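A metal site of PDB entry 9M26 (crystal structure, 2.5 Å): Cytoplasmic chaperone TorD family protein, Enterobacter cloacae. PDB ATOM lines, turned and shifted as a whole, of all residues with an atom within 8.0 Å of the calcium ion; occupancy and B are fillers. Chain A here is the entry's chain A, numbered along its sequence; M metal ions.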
ATOM      1  N   GLU A 138      -5.936 -11.297 -27.846  1.00  0.00           N
ATOM      2  CA  GLU A 138      -5.030 -10.155 -27.987  1.00  0.00           C
ATOM      3  C   GLU A 138      -3.625 -10.607 -28.372  1.00  0.00           C
ATOM      4  O   GLU A 138      -2.973  -9.986 -29.210  1.00  0.00           O
ATOM      5  CB  GLU A 138      -4.983  -9.337 -26.695  1.00  0.00           C
ATOM      6  CG  GLU A 138      -4.193  -8.047 -26.829  1.00  0.00           C
ATOM      7  CD  GLU A 138      -3.950  -7.336 -25.506  1.00  0.00           C
ATOM      8  OE1 GLU A 138      -2.942  -7.658 -24.834  1.00  0.00           O
ATOM      9  OE2 GLU A 138      -4.767  -6.477 -25.133  1.00  0.00           O
ATOM     10  N   THR A 139      -3.160 -11.705 -27.771  1.00  0.00           N
ATOM     11  CA  THR A 139      -1.837 -12.214 -28.109  1.00  0.00           C
ATOM     12  C   THR A 139      -1.791 -12.756 -29.533  1.00  0.00           C
ATOM     13  O   THR A 139      -0.820 -12.523 -30.267  1.00  0.00           O
ATOM     14  CB  THR A 139      -1.411 -13.261 -27.080  1.00  0.00           C
ATOM     15  OG1 THR A 139      -1.338 -12.644 -25.794  1.00  0.00           O
ATOM     16  CG2 THR A 139      -0.050 -13.851 -27.429  1.00  0.00           C
ATOM     17  N   GLU A 142      -1.794  -9.413 -31.689  1.00  0.00           N
ATOM     18  CA  GLU A 142      -0.679  -8.489 -31.486  1.00  0.00           C
ATOM     19  C   GLU A 142       0.657  -9.131 -31.830  1.00  0.00           C
ATOM     20  O   GLU A 142       1.549  -8.457 -32.354  1.00  0.00           O
ATOM     21  CB  GLU A 142      -0.681  -7.949 -30.046  1.00  0.00           C
ATOM     22  CG  GLU A 142      -1.223  -6.550 -29.973  1.00  0.00           C
ATOM     23  CD  GLU A 142      -1.433  -6.018 -28.566  1.00  0.00           C
ATOM     24  OE1 GLU A 142      -1.934  -4.886 -28.448  1.00  0.00           O
ATOM     25  OE2 GLU A 142      -1.113  -6.722 -27.595  1.00  0.00           O
ATOM     26  N   TRP A 180      -9.718  -5.582 -35.290  1.00  0.00           N
ATOM     27  CA  TRP A 180      -8.706  -5.209 -34.299  1.00  0.00           C
ATOM     28  C   TRP A 180      -9.082  -3.925 -33.565  1.00  0.00           C
ATOM     29  O   TRP A 180      -8.871  -3.817 -32.350  1.00  0.00           O
ATOM     30  CB  TRP A 180      -7.338  -5.077 -34.956  1.00  0.00           C
ATOM     31  CG  TRP A 180      -6.257  -4.802 -33.969  1.00  0.00           C
ATOM     32  CD1 TRP A 180      -5.382  -3.741 -33.965  1.00  0.00           C
ATOM     33  CD2 TRP A 180      -5.958  -5.560 -32.788  1.00  0.00           C
ATOM     34  NE1 TRP A 180      -4.527  -3.834 -32.886  1.00  0.00           N
ATOM     35  CE2 TRP A 180      -4.866  -4.940 -32.142  1.00  0.00           C
ATOM     36  CE3 TRP A 180      -6.489  -6.732 -32.228  1.00  0.00           C
ATOM     37  CZ2 TRP A 180      -4.301  -5.445 -30.978  1.00  0.00           C
ATOM     38  CZ3 TRP A 180      -5.935  -7.220 -31.051  1.00  0.00           C
ATOM     39  CH2 TRP A 180      -4.855  -6.580 -30.451  1.00  0.00           C
ATOM     40  N   LEU A 183     -11.679  -4.924 -30.898  1.00  0.00           N
ATOM     41  CA  LEU A 183     -11.047  -5.657 -29.800  1.00  0.00           C
ATOM     42  C   LEU A 183     -10.183  -4.745 -28.935  1.00  0.00           C
ATOM     43  O   LEU A 183     -10.263  -4.772 -27.704  1.00  0.00           O
ATOM     44  CB  LEU A 183     -10.228  -6.831 -30.347  1.00  0.00           C
ATOM     45  CG  LEU A 183     -11.020  -7.846 -31.182  1.00  0.00           C
ATOM     46  CD1 LEU A 183     -10.109  -8.659 -32.096  1.00  0.00           C
ATOM     47  CD2 LEU A 183     -11.837  -8.753 -30.291  1.00  0.00           C
ATOM     48  N   GLU A 184      -9.319  -3.943 -29.576  1.00  0.00           N
ATOM     49  CA  GLU A 184      -8.437  -3.058 -28.817  1.00  0.00           C
ATOM     50  C   GLU A 184      -9.235  -2.070 -27.986  1.00  0.00           C
ATOM     51  O   GLU A 184      -8.795  -1.711 -26.880  1.00  0.00           O
ATOM     52  CB  GLU A 184      -7.489  -2.302 -29.732  1.00  0.00           C
ATOM     53  CG  GLU A 184      -6.153  -2.971 -29.924  1.00  0.00           C
ATOM     54  CD  GLU A 184      -5.382  -3.196 -28.629  1.00  0.00           C
ATOM     55  OE1 GLU A 184      -5.666  -4.185 -27.925  1.00  0.00           O
ATOM     56  OE2 GLU A 184      -4.470  -2.399 -28.323  1.00  0.00           O
ATOM     57  N   GLU A 185     -10.408  -1.631 -28.469  1.00  0.00           N
ATOM     58  CA  GLU A 185     -11.197  -0.690 -27.694  1.00  0.00           C
ATOM     59  C   GLU A 185     -11.679  -1.322 -26.393  1.00  0.00           C
ATOM     60  O   GLU A 185     -11.903  -0.622 -25.406  1.00  0.00           O
ATOM     61  CB  GLU A 185     -12.402  -0.192 -28.497  1.00  0.00           C
ATOM     62  CG  GLU A 185     -12.094   0.856 -29.554  1.00  0.00           C
ATOM     63  CD  GLU A 185     -13.190   0.966 -30.609  1.00  0.00           C
ATOM     64  OE1 GLU A 185     -14.057   0.076 -30.681  1.00  0.00           O
ATOM     65  OE2 GLU A 185     -13.197   1.967 -31.358  1.00  0.00           O
ATOM     66  N   GLU A 186     -11.800  -2.648 -26.375  1.00  0.00           N
ATOM     67  CA  GLU A 186     -12.135  -3.370 -25.157  1.00  0.00           C
ATOM     68  C   GLU A 186     -10.898  -3.814 -24.396  1.00  0.00           C
ATOM     69  O   GLU A 186     -10.927  -3.873 -23.157  1.00  0.00           O
ATOM     70  CB  GLU A 186     -12.997  -4.598 -25.493  1.00  0.00           C
ATOM     71  CG  GLU A 186     -14.307  -4.255 -26.213  1.00  0.00           C
ATOM     72  CD  GLU A 186     -15.067  -3.109 -25.549  1.00  0.00           C
ATOM     73  OE1 GLU A 186     -15.563  -3.264 -24.411  1.00  0.00           O
ATOM     74  OE2 GLU A 186     -15.147  -2.027 -26.159  1.00  0.00           O
ATOM     75  N   ASN A 187      -9.801  -4.133 -25.105  1.00  0.00           N
ATOM     76  CA  ASN A 187      -8.561  -4.526 -24.444  1.00  0.00           C
ATOM     77  C   ASN A 187      -7.989  -3.390 -23.628  1.00  0.00           C
ATOM     78  O   ASN A 187      -7.538  -3.588 -22.496  1.00  0.00           O
ATOM     79  CB  ASN A 187      -7.531  -4.975 -25.485  1.00  0.00           C
ATOM     80  CG  ASN A 187      -7.896  -6.267 -26.171  1.00  0.00           C
ATOM     81  OD1 ASN A 187      -8.776  -7.010 -25.719  1.00  0.00           O
ATOM     82  ND2 ASN A 187      -7.190  -6.576 -27.262  1.00  0.00           N
ATOM     83  N   GLU A 188      -7.976  -2.188 -24.209  1.00  0.00           N
ATOM     84  CA  GLU A 188      -7.379  -1.016 -23.603  1.00  0.00           C
ATOM     85  C   GLU A 188      -8.416  -0.080 -23.011  1.00  0.00           C
ATOM     86  O   GLU A 188      -8.131   1.100 -22.800  1.00  0.00           O
ATOM     87  CB  GLU A 188      -6.535  -0.259 -24.646  1.00  0.00           C
ATOM     88  CG  GLU A 188      -5.607  -1.144 -25.453  1.00  0.00           C
ATOM     89  CD  GLU A 188      -4.634  -1.911 -24.577  1.00  0.00           C
ATOM     90  OE1 GLU A 188      -4.208  -1.350 -23.540  1.00  0.00           O
ATOM     91  OE2 GLU A 188      -4.318  -3.078 -24.920  1.00  0.00           O
HETATM   92 CA    CA M   1      -3.435  -4.300 -26.794  1.00  0.00          CA
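The calcium ion is bound by OE1 of Glu 142 (2.3 Å).
The side-chain carboxylate (OE2) of Glu 188 binds the calcium ion (2.4 Å).
OE1 of Glu 184 binds the calcium ion (2.5 Å).
The calcium ion is bound by OE2 of Glu 184, 2.7 Å away.
Slightly farther from the calcium ion lies OE2 of Glu 138 (3.0 Å).
OE1 of Glu 184 sits close to ND2 of Asn 187.
The side-chain carboxylate of Glu 138 sits close to the side-chain amide nitrogen of Asn 187 (3.2 Å).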
